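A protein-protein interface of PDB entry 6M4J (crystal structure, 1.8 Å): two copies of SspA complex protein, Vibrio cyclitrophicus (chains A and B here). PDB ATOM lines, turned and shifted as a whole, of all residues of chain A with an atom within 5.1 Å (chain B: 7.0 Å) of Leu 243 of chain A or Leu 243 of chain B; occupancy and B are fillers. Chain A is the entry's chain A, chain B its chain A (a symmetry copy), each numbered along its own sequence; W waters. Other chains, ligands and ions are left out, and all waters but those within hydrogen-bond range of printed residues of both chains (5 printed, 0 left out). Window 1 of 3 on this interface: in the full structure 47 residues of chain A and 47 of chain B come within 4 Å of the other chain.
Among the printed residues, pairs that only touch across the chains: Lys 206 of chain A with Pro 240 of chain B (3.8 Å), Pro 240 of chain A with Lys 206 of chain B (3.8 Å), Lys 206 of chain A with Leu 243 of chain B (3.9 Å), Leu 243 of chain A with Lys 206 of chain B (3.9 Å), Gly 207 of chain A with Pro 240 of chain B (3.9 Å), Pro 240 of chain A with Gly 207 of chain B (3.9 Å) and Leu 243 of chain A with Leu 243 of chain B (3.98 Å).
Of chain A, only Lys 206 and Leu 243 come within 4 Å of Leu 243 of chain B.
Printed residues of chain B within 4 Å of Lys 206 of chain A: Pro 240 (3.8 Å) and Leu 243 (3.9 Å).
Of the printed residues of chain B, Pro 240 of chain A touches Lys 206 and Gly 207.
Of the printed residues of chain A, Gly 207 of chain B touches Pro 240.
Of the printed residues of chain A, Pro 240 of chain B touches Lys 206 and Gly 207.
The nearest residue of chain B that does not touch Leu 243 of chain A is Gly 207 of chain B (4.1 Å).
The nearest residue of chain A that does not touch Leu 243 of chain B is Gly 207 of chain A (4.1 Å).
Of the 13 printed residues of chain A, 4 touch a printed residue of chain B.
Hydrophobic or aromatic side chains of chain A that line the printed part of chain B: Pro 240 and Leu 243.
Along chain B the printed residues that touch a printed residue of chain A span positions 206 to 243.
Lys 206 of chain A touches Pro 240 of chain B, and with the chains exchanged Pro 240 of chain A touches Lys 206 of chain B.
Lys 206 of chain A touches Leu 243 of chain B, and with the chains exchanged Leu 243 of chain A touches Lys 206 of chain B.
Gly 207 of chain A touches Pro 240 of chain B, and with the chains exchanged Pro 240 of chain A touches Gly 207 of chain B.
Leu 243 of chain B touches its own counterpart, Leu 243 of chain A.
Of the 7 pairs that touch across the chains among the printed residues, 7 have their exchanged pair printed and touching as well.
Water W4 lies within hydrogen-bond range of the backbone carbonyl oxygen of Gly 207 of chain B (2.7 Å) and the backbone carbonyl oxygen of Gly 207 of chain A (3.2 Å).
Water W1 lies within hydrogen-bond range of O of Gly 207 of chain A (2.7 Å) and O of Gly 207 of chain B (3.2 Å).
Water W3 lies within hydrogen-bond range of O of Trp 24 of chain B (2.8 Å) and NZ of Lys 206 of chain A (2.8 Å).
Water W5 lies within hydrogen-bond range of NE2 of Gln 25 of chain B (2.8 Å) and N of Lys 206 of chain A (2.9 Å).
Water W2 bridges the backbone carbonyl oxygen (O) of Trp 24 of chain B (2.9 Å) and the side-chain amino group (NZ) of Lys 206 of chain A (3.0 Å).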
ATOM      1  N   MET A  21       9.770 -34.161  17.852  1.00  0.00           N
ATOM      2  CA  MET A  21       8.518 -33.459  17.594  1.00  0.00           C
ATOM      3  C   MET A  21       7.300 -34.284  17.916  1.00  0.00           C
ATOM      4  O   MET A  21       6.261 -33.719  18.229  1.00  0.00           O
ATOM      5  CB  MET A  21       8.444 -32.950  16.155  1.00  0.00           C
ATOM      6  CG  MET A  21       9.441 -31.843  15.904  1.00  0.00           C
ATOM      7  SD  MET A  21       9.234 -31.079  14.290  1.00  0.00           S
ATOM      8  CE  MET A  21       9.948 -32.370  13.308  1.00  0.00           C
ATOM      9  N   PRO A 205      12.943 -28.446  11.379  1.00  0.00           N
ATOM     10  CA  PRO A 205      11.714 -28.383  10.621  1.00  0.00           C
ATOM     11  C   PRO A 205      11.497 -27.020   9.980  1.00  0.00           C
ATOM     12  O   PRO A 205      12.068 -26.005  10.408  1.00  0.00           O
ATOM     13  CB  PRO A 205      10.630 -28.677  11.659  1.00  0.00           C
ATOM     14  CG  PRO A 205      11.218 -28.240  12.945  1.00  0.00           C
ATOM     15  CD  PRO A 205      12.706 -28.407  12.834  1.00  0.00           C
ATOM     16  N   LYS A 206      10.681 -27.023   8.933  1.00  0.00           N
ATOM     17  CA  LYS A 206      10.186 -25.787   8.350  1.00  0.00           C
ATOM     18  C   LYS A 206       9.169 -25.127   9.287  1.00  0.00           C
ATOM     19  O   LYS A 206       8.523 -25.796  10.118  1.00  0.00           O
ATOM     20  CB  LYS A 206       9.571 -26.041   6.962  1.00  0.00           C
ATOM     21  CG  LYS A 206      10.620 -26.290   5.884  1.00  0.00           C
ATOM     22  CD  LYS A 206       9.996 -26.599   4.527  1.00  0.00           C
ATOM     23  CE  LYS A 206      11.072 -26.991   3.507  1.00  0.00           C
ATOM     24  NZ  LYS A 206      11.697 -28.321   3.803  1.00  0.00           N
ATOM     25  N   GLY A 207       9.040 -23.809   9.143  1.00  0.00           N
ATOM     26  CA  GLY A 207       8.125 -23.010   9.947  1.00  0.00           C
ATOM     27  C   GLY A 207       8.657 -22.536  11.283  1.00  0.00           C
ATOM     28  O   GLY A 207       7.886 -22.032  12.094  1.00  0.00           O
ATOM     29  N   ILE A 208       9.968 -22.639  11.507  1.00  0.00           N
ATOM     30  CA  ILE A 208      10.539 -22.100  12.737  1.00  0.00           C
ATOM     31  C   ILE A 208      11.880 -21.409  12.510  1.00  0.00           C
ATOM     32  O   ILE A 208      12.653 -21.826  11.682  1.00  0.00           O
ATOM     33  CB  ILE A 208      10.664 -23.217  13.787  1.00  0.00           C
ATOM     34  CG1 ILE A 208      10.923 -22.642  15.181  1.00  0.00           C
ATOM     35  CG2 ILE A 208      11.702 -24.246  13.374  1.00  0.00           C
ATOM     36  CD1 ILE A 208       9.693 -22.004  15.783  1.00  0.00           C
ATOM     37  N   PRO A 240       4.755 -22.741  19.013  1.00  0.00           N
ATOM     38  CA  PRO A 240       4.562 -24.062  18.394  1.00  0.00           C
ATOM     39  C   PRO A 240       5.531 -25.108  18.942  1.00  0.00           C
ATOM     40  O   PRO A 240       6.597 -25.348  18.359  1.00  0.00           O
ATOM     41  CB  PRO A 240       4.830 -23.779  16.915  1.00  0.00           C
ATOM     42  CG  PRO A 240       5.831 -22.662  16.935  1.00  0.00           C
ATOM     43  CD  PRO A 240       5.439 -21.794  18.109  1.00  0.00           C
ATOM     44  N   THR A 241       5.137 -25.757  20.034  1.00  0.00           N
ATOM     45  CA  THR A 241       6.103 -26.511  20.810  1.00  0.00           C
ATOM     46  C   THR A 241       6.843 -27.575  20.014  1.00  0.00           C
ATOM     47  O   THR A 241       8.032 -27.644  20.127  1.00  0.00           O
ATOM     48  CB  THR A 241       5.612 -26.879  22.241  1.00  0.00           C
ATOM     49  OG1 THR A 241       6.052 -28.182  22.700  1.00  0.00           O
ATOM     50  CG2 THR A 241       4.151 -26.619  22.432  1.00  0.00           C
ATOM     51  N   PRO A 242       6.161 -28.327  19.146  1.00  0.00           N
ATOM     52  CA  PRO A 242       6.919 -29.320  18.372  1.00  0.00           C
ATOM     53  C   PRO A 242       8.050 -28.707  17.533  1.00  0.00           C
ATOM     54  O   PRO A 242       9.174 -29.230  17.517  1.00  0.00           O
ATOM     55  CB  PRO A 242       5.859 -29.962  17.459  1.00  0.00           C
ATOM     56  CG  PRO A 242       4.526 -29.546  18.013  1.00  0.00           C
ATOM     57  CD  PRO A 242       4.752 -28.248  18.749  1.00  0.00           C
ATOM     58  N   LEU A 243       7.762 -27.593  16.858  1.00  0.00           N
ATOM     59  CA  LEU A 243       8.762 -26.892  16.019  1.00  0.00           C
ATOM     60  C   LEU A 243       9.934 -26.328  16.839  1.00  0.00           C
ATOM     61  O   LEU A 243      11.109 -26.413  16.442  1.00  0.00           O
ATOM     62  CB  LEU A 243       8.089 -25.770  15.226  1.00  0.00           C
ATOM     63  CG  LEU A 243       6.979 -26.226  14.277  1.00  0.00           C
ATOM     64  CD1 LEU A 243       6.278 -25.008  13.702  1.00  0.00           C
ATOM     65  CD2 LEU A 243       7.528 -27.109  13.159  1.00  0.00           C
ATOM     66  N   ILE A 244       9.609 -25.773  18.004  1.00  0.00           N
ATOM     67  CA  ILE A 244      10.630 -25.240  18.893  1.00  0.00           C
ATOM     68  C   ILE A 244      11.541 -26.366  19.422  1.00  0.00           C
ATOM     69  O   ILE A 244      12.775 -26.267  19.354  1.00  0.00           O
ATOM     70  CB  ILE A 244       9.978 -24.458  20.054  1.00  0.00           C
ATOM     71  CG1 ILE A 244       9.418 -23.109  19.573  1.00  0.00           C
ATOM     72  CG2 ILE A 244      10.993 -24.161  21.138  1.00  0.00           C
ATOM     73  CD1 ILE A 244       8.371 -22.512  20.502  1.00  0.00           C
ATOM     74  N   VAL A 245      10.924 -27.437  19.923  1.00  0.00           N
ATOM     75  CA  VAL A 245      11.668 -28.614  20.393  1.00  0.00           C
ATOM     76  C   VAL A 245      12.576 -29.174  19.281  1.00  0.00           C
ATOM     77  O   VAL A 245      13.756 -29.440  19.504  1.00  0.00           O
ATOM     78  CB  VAL A 245      10.708 -29.686  20.987  1.00  0.00           C
ATOM     79  CG1 VAL A 245      11.417 -31.003  21.261  1.00  0.00           C
ATOM     80  CG2 VAL A 245      10.074 -29.177  22.279  1.00  0.00           C
ATOM     81  N   GLY A 246      12.035 -29.302  18.076  1.00  0.00           N
ATOM     82  CA  GLY A 246      12.794 -29.849  16.962  1.00  0.00           C
ATOM     83  C   GLY A 246      13.978 -28.974  16.615  1.00  0.00           C
ATOM     84  O   GLY A 246      15.044 -29.488  16.274  1.00  0.00           O
ATOM     85  N   LEU A 247      13.797 -27.658  16.711  1.00  0.00           N
ATOM     86  CA  LEU A 247      14.886 -26.739  16.421  1.00  0.00           C
ATOM     87  C   LEU A 247      16.034 -26.915  17.417  1.00  0.00           C
ATOM     88  O   LEU A 247      17.207 -26.934  17.029  1.00  0.00           O
ATOM     89  CB  LEU A 247      14.390 -25.292  16.400  1.00  0.00           C
ATOM     90  CG  LEU A 247      15.458 -24.229  16.120  1.00  0.00           C
ATOM     91  CD1 LEU A 247      16.229 -24.486  14.823  1.00  0.00           C
ATOM     92  CD2 LEU A 247      14.796 -22.857  16.096  1.00  0.00           C
ATOM     93  N   VAL B  17      -3.512 -36.186   9.917  1.00  0.00           N
ATOM     94  CA  VAL B  17      -2.711 -34.977   9.780  1.00  0.00           C
ATOM     95  C   VAL B  17      -1.240 -35.294  10.024  1.00  0.00           C
ATOM     96  O   VAL B  17      -0.386 -34.971   9.211  1.00  0.00           O
ATOM     97  CB  VAL B  17      -3.195 -33.878  10.747  1.00  0.00           C
ATOM     98  CG1 VAL B  17      -2.268 -32.664  10.706  1.00  0.00           C
ATOM     99  CG2 VAL B  17      -4.635 -33.489  10.426  1.00  0.00           C
ATOM    100  N   MET B  21       1.974 -35.180   7.170  1.00  0.00           N
ATOM    101  CA  MET B  21       3.163 -34.352   7.326  1.00  0.00           C
ATOM    102  C   MET B  21       4.446 -35.112   7.110  1.00  0.00           C
ATOM    103  O   MET B  21       5.438 -34.511   6.719  1.00  0.00           O
ATOM    104  CB  MET B  21       3.188 -33.655   8.686  1.00  0.00           C
ATOM    105  CG  MET B  21       2.105 -32.608   8.795  1.00  0.00           C
ATOM    106  SD  MET B  21       2.241 -31.625  10.294  1.00  0.00           S
ATOM    107  CE  MET B  21       1.628 -32.829  11.440  1.00  0.00           C
ATOM    108  N   TRP B  24       7.164 -35.051   4.112  1.00  0.00           N
ATOM    109  CA  TRP B  24       7.730 -33.745   3.785  1.00  0.00           C
ATOM    110  C   TRP B  24       8.744 -33.281   4.770  1.00  0.00           C
ATOM    111  O   TRP B  24       9.169 -32.128   4.726  1.00  0.00           O
ATOM    112  CB  TRP B  24       6.632 -32.701   3.674  1.00  0.00           C
ATOM    113  CG  TRP B  24       5.579 -33.091   2.682  1.00  0.00           C
ATOM    114  CD1 TRP B  24       4.316 -33.610   2.948  1.00  0.00           C
ATOM    115  CD2 TRP B  24       5.692 -33.068   1.222  1.00  0.00           C
ATOM    116  NE1 TRP B  24       3.644 -33.871   1.780  1.00  0.00           N
ATOM    117  CE2 TRP B  24       4.417 -33.570   0.706  1.00  0.00           C
ATOM    118  CE3 TRP B  24       6.677 -32.672   0.320  1.00  0.00           C
ATOM    119  CZ2 TRP B  24       4.163 -33.668  -0.654  1.00  0.00           C
ATOM    120  CZ3 TRP B  24       6.412 -32.779  -1.052  1.00  0.00           C
ATOM    121  CH2 TRP B  24       5.188 -33.265  -1.524  1.00  0.00           C
ATOM    122  N   GLN B  25       9.161 -34.192   5.638  1.00  0.00           N
ATOM    123  CA  GLN B  25      10.181 -33.900   6.618  1.00  0.00           C
ATOM    124  C   GLN B  25      11.569 -34.231   6.082  1.00  0.00           C
ATOM    125  O   GLN B  25      12.412 -33.355   5.964  1.00  0.00           O
ATOM    126  CB  GLN B  25       9.885 -34.636   7.930  1.00  0.00           C
ATOM    127  CG  GLN B  25       8.457 -34.460   8.468  1.00  0.00           C
ATOM    128  CD  GLN B  25       8.196 -33.126   9.155  1.00  0.00           C
ATOM    129  OE1 GLN B  25       7.104 -32.903   9.681  1.00  0.00           O
ATOM    130  NE2 GLN B  25       9.185 -32.237   9.156  1.00  0.00           N
ATOM    131  N   ALA B  49      -3.949 -28.239  -0.514  1.00  0.00           N
ATOM    132  CA  ALA B  49      -4.395 -27.740   0.780  1.00  0.00           C
ATOM    133  C   ALA B  49      -5.084 -26.374   0.642  1.00  0.00           C
ATOM    134  O   ALA B  49      -6.148 -26.114   1.223  1.00  0.00           O
ATOM    135  CB  ALA B  49      -3.207 -27.649   1.720  1.00  0.00           C
ATOM    136  N   PHE B  66      -1.283 -18.124   3.383  1.00  0.00           N
ATOM    137  CA  PHE B  66      -0.800 -18.851   4.553  1.00  0.00           C
ATOM    138  C   PHE B  66      -0.015 -17.971   5.524  1.00  0.00           C
ATOM    139  O   PHE B  66       0.702 -17.057   5.112  1.00  0.00           O
ATOM    140  CB  PHE B  66      -0.001 -20.088   4.156  1.00  0.00           C
ATOM    141  CG  PHE B  66      -0.837 -21.150   3.521  1.00  0.00           C
ATOM    142  CD1 PHE B  66      -0.688 -21.455   2.177  1.00  0.00           C
ATOM    143  CD2 PHE B  66      -1.799 -21.832   4.255  1.00  0.00           C
ATOM    144  CE1 PHE B  66      -1.476 -22.437   1.580  1.00  0.00           C
ATOM    145  CE2 PHE B  66      -2.582 -22.813   3.668  1.00  0.00           C
ATOM    146  CZ  PHE B  66      -2.431 -23.115   2.323  1.00  0.00           C
ATOM    147  N   CYS B  68       1.424 -18.054  10.033  1.00  0.00           N
ATOM    148  CA  CYS B  68       1.484 -19.039  11.024  1.00  0.00           C
ATOM    149  C   CYS B  68       0.409 -19.234  12.044  1.00  0.00           C
ATOM    150  O   CYS B  68       0.552 -20.058  12.929  1.00  0.00           O
ATOM    151  CB  CYS B  68       2.753 -18.990  11.783  1.00  0.00           C
ATOM    152  SG  CYS B  68       2.825 -17.599  12.902  1.00  0.00           S
ATOM    153  N   GLY B 204      -5.278 -29.434  13.565  1.00  0.00           N
ATOM    154  CA  GLY B 204      -4.097 -29.246  12.718  1.00  0.00           C
ATOM    155  C   GLY B 204      -2.834 -29.014  13.534  1.00  0.00           C
ATOM    156  O   GLY B 204      -2.888 -28.876  14.770  1.00  0.00           O
ATOM    157  N   PRO B 205      -1.683 -28.940  12.854  1.00  0.00           N
ATOM    158  CA  PRO B 205      -0.467 -28.679  13.591  1.00  0.00           C
ATOM    159  C   PRO B 205      -0.364 -27.231  14.046  1.00  0.00           C
ATOM    160  O   PRO B 205      -1.012 -26.330  13.492  1.00  0.00           O
ATOM    161  CB  PRO B 205       0.643 -29.019  12.594  1.00  0.00           C
ATOM    162  CG  PRO B 205       0.029 -28.803  11.266  1.00  0.00           C
ATOM    163  CD  PRO B 205      -1.442 -29.073  11.406  1.00  0.00           C
ATOM    164  N   LYS B 206       0.444 -27.031  15.081  1.00  0.00           N
ATOM    165  CA  LYS B 206       0.835 -25.693  15.494  1.00  0.00           C
ATOM    166  C   LYS B 206       1.801 -25.083  14.473  1.00  0.00           C
ATOM    167  O   LYS B 206       2.503 -25.801  13.733  1.00  0.00           O
ATOM    168  CB  LYS B 206       1.462 -25.714  16.900  1.00  0.00           C
ATOM    169  CG  LYS B 206       0.430 -25.902  18.007  1.00  0.00           C
ATOM    170  CD  LYS B 206       1.070 -25.980  19.390  1.00  0.00           C
ATOM    171  CE  LYS B 206       0.024 -26.320  20.458  1.00  0.00           C
ATOM    172  NZ  LYS B 206      -0.491 -27.723  20.342  1.00  0.00           N
ATOM    173  N   GLY B 207       1.823 -23.751  14.442  1.00  0.00           N
ATOM    174  CA  GLY B 207       2.676 -22.994  13.536  1.00  0.00           C
ATOM    175  C   GLY B 207       2.114 -22.743  12.152  1.00  0.00           C
ATOM    176  O   GLY B 207       2.847 -22.289  11.278  1.00  0.00           O
ATOM    177  N   ILE B 208       0.816 -22.979  11.950  1.00  0.00           N
ATOM    178  CA  ILE B 208       0.210 -22.654  10.664  1.00  0.00           C
ATOM    179  C   ILE B 208      -1.183 -22.049  10.805  1.00  0.00           C
ATOM    180  O   ILE B 208      -1.924 -22.415  11.685  1.00  0.00           O
ATOM    181  CB  ILE B 208       0.181 -23.906   9.769  1.00  0.00           C
ATOM    182  CG1 ILE B 208      -0.116 -23.540   8.314  1.00  0.00           C
ATOM    183  CG2 ILE B 208      -0.773 -24.951  10.319  1.00  0.00           C
ATOM    184  CD1 ILE B 208       1.063 -22.890   7.626  1.00  0.00           C
ATOM    185  N   GLY B 209      -1.533 -21.117   9.941  1.00  0.00           N
ATOM    186  CA  GLY B 209      -2.915 -20.682   9.858  1.00  0.00           C
ATOM    187  C   GLY B 209      -3.079 -20.042   8.500  1.00  0.00           C
ATOM    188  O   GLY B 209      -2.276 -20.284   7.592  1.00  0.00           O
ATOM    189  N   PRO B 240       6.061 -23.646   4.495  1.00  0.00           N
ATOM    190  CA  PRO B 240       6.356 -24.854   5.281  1.00  0.00           C
ATOM    191  C   PRO B 240       5.477 -26.037   4.880  1.00  0.00           C
ATOM    192  O   PRO B 240       4.431 -26.284   5.495  1.00  0.00           O
ATOM    193  CB  PRO B 240       6.059 -24.403   6.711  1.00  0.00           C
ATOM    194  CG  PRO B 240       4.971 -23.382   6.551  1.00  0.00           C
ATOM    195  CD  PRO B 240       5.298 -22.647   5.270  1.00  0.00           C
ATOM    196  N   THR B 241       5.927 -26.790   3.880  1.00  0.00           N
ATOM    197  CA  THR B 241       5.030 -27.715   3.215  1.00  0.00           C
ATOM    198  C   THR B 241       4.373 -28.721   4.147  1.00  0.00           C
ATOM    199  O   THR B 241       3.194 -28.899   4.051  1.00  0.00           O
ATOM    200  CB  THR B 241       5.556 -28.226   1.841  1.00  0.00           C
ATOM    201  OG1 THR B 241       5.225 -29.609   1.560  1.00  0.00           O
ATOM    202  CG2 THR B 241       6.992 -27.877   1.610  1.00  0.00           C
ATOM    203  N   PRO B 242       5.109 -29.295   5.102  1.00  0.00           N
ATOM    204  CA  PRO B 242       4.429 -30.236   6.004  1.00  0.00           C
ATOM    205  C   PRO B 242       3.248 -29.611   6.761  1.00  0.00           C
ATOM    206  O   PRO B 242       2.169 -30.216   6.852  1.00  0.00           O
ATOM    207  CB  PRO B 242       5.532 -30.665   6.987  1.00  0.00           C
ATOM    208  CG  PRO B 242       6.831 -30.220   6.377  1.00  0.00           C
ATOM    209  CD  PRO B 242       6.505 -29.052   5.478  1.00  0.00           C
ATOM    210  N   LEU B 243       3.442 -28.399   7.283  1.00  0.00           N
ATOM    211  CA  LEU B 243       2.384 -27.677   8.029  1.00  0.00           C
ATOM    212  C   LEU B 243       1.176 -27.321   7.148  1.00  0.00           C
ATOM    213  O   LEU B 243       0.009 -27.448   7.558  1.00  0.00           O
ATOM    214  CB  LEU B 243       2.961 -26.410   8.664  1.00  0.00           C
ATOM    215  CG  LEU B 243       4.098 -26.646   9.659  1.00  0.00           C
ATOM    216  CD1 LEU B 243       4.697 -25.312  10.065  1.00  0.00           C
ATOM    217  CD2 LEU B 243       3.617 -27.416  10.886  1.00  0.00           C
ATOM    218  N   ILE B 244       1.460 -26.899   5.919  1.00  0.00           N
ATOM    219  CA  ILE B 244       0.404 -26.571   4.973  1.00  0.00           C
ATOM    220  C   ILE B 244      -0.410 -27.826   4.601  1.00  0.00           C
ATOM    221  O   ILE B 244      -1.648 -27.819   4.661  1.00  0.00           O
ATOM    222  CB  ILE B 244       0.998 -25.898   3.715  1.00  0.00           C
ATOM    223  CG1 ILE B 244       1.445 -24.457   4.013  1.00  0.00           C
ATOM    224  CG2 ILE B 244      -0.032 -25.828   2.607  1.00  0.00           C
ATOM    225  CD1 ILE B 244       2.446 -23.905   3.008  1.00  0.00           C
ATOM    226  N   VAL B 245       0.294 -28.901   4.241  1.00  0.00           N
ATOM    227  CA  VAL B 245      -0.351 -30.185   3.933  1.00  0.00           C
ATOM    228  C   VAL B 245      -1.217 -30.665   5.114  1.00  0.00           C
ATOM    229  O   VAL B 245      -2.370 -31.053   4.934  1.00  0.00           O
ATOM    230  CB  VAL B 245       0.696 -31.244   3.480  1.00  0.00           C
ATOM    231  CG1 VAL B 245       0.096 -32.639   3.384  1.00  0.00           C
ATOM    232  CG2 VAL B 245       1.294 -30.860   2.129  1.00  0.00           C
ATOM    233  N   GLY B 246      -0.674 -30.591   6.322  1.00  0.00           N
ATOM    234  CA  GLY B 246      -1.392 -31.045   7.502  1.00  0.00           C
ATOM    235  C   GLY B 246      -2.645 -30.231   7.738  1.00  0.00           C
ATOM    236  O   GLY B 246      -3.667 -30.780   8.149  1.00  0.00           O
ATOM    237  N   LEU B 247      -2.569 -28.929   7.470  1.00  0.00           N
ATOM    238  CA  LEU B 247      -3.730 -28.069   7.643  1.00  0.00           C
ATOM    239  C   LEU B 247      -4.855 -28.467   6.684  1.00  0.00           C
ATOM    240  O   LEU B 247      -6.024 -28.528   7.078  1.00  0.00           O
ATOM    241  CB  LEU B 247      -3.352 -26.597   7.471  1.00  0.00           C
ATOM    242  CG  LEU B 247      -4.504 -25.596   7.614  1.00  0.00           C
ATOM    243  CD1 LEU B 247      -5.258 -25.742   8.938  1.00  0.00           C
ATOM    244  CD2 LEU B 247      -3.954 -24.184   7.455  1.00  0.00           C
ATOM    245  N   GLY B 248      -4.500 -28.765   5.437  1.00  0.00           N
ATOM    246  CA  GLY B 248      -5.504 -29.230   4.482  1.00  0.00           C
ATOM    247  C   GLY B 248      -6.199 -30.503   4.943  1.00  0.00           C
ATOM    248  O   GLY B 248      -7.419 -30.644   4.801  1.00  0.00           O
HETATM  249  O   HOH W   1       5.423 -21.258  12.937  1.00  0.00           O
HETATM  250  O   HOH W   2      10.884 -30.164   6.071  1.00  0.00           O
HETATM  251  O   HOH W   3       9.347 -29.766   3.324  1.00  0.00           O
HETATM  252  O   HOH W   4       5.244 -21.438  10.327  1.00  0.00           O
HETATM  253  O   HOH W   5       9.574 -29.620   8.297  1.00  0.00           O
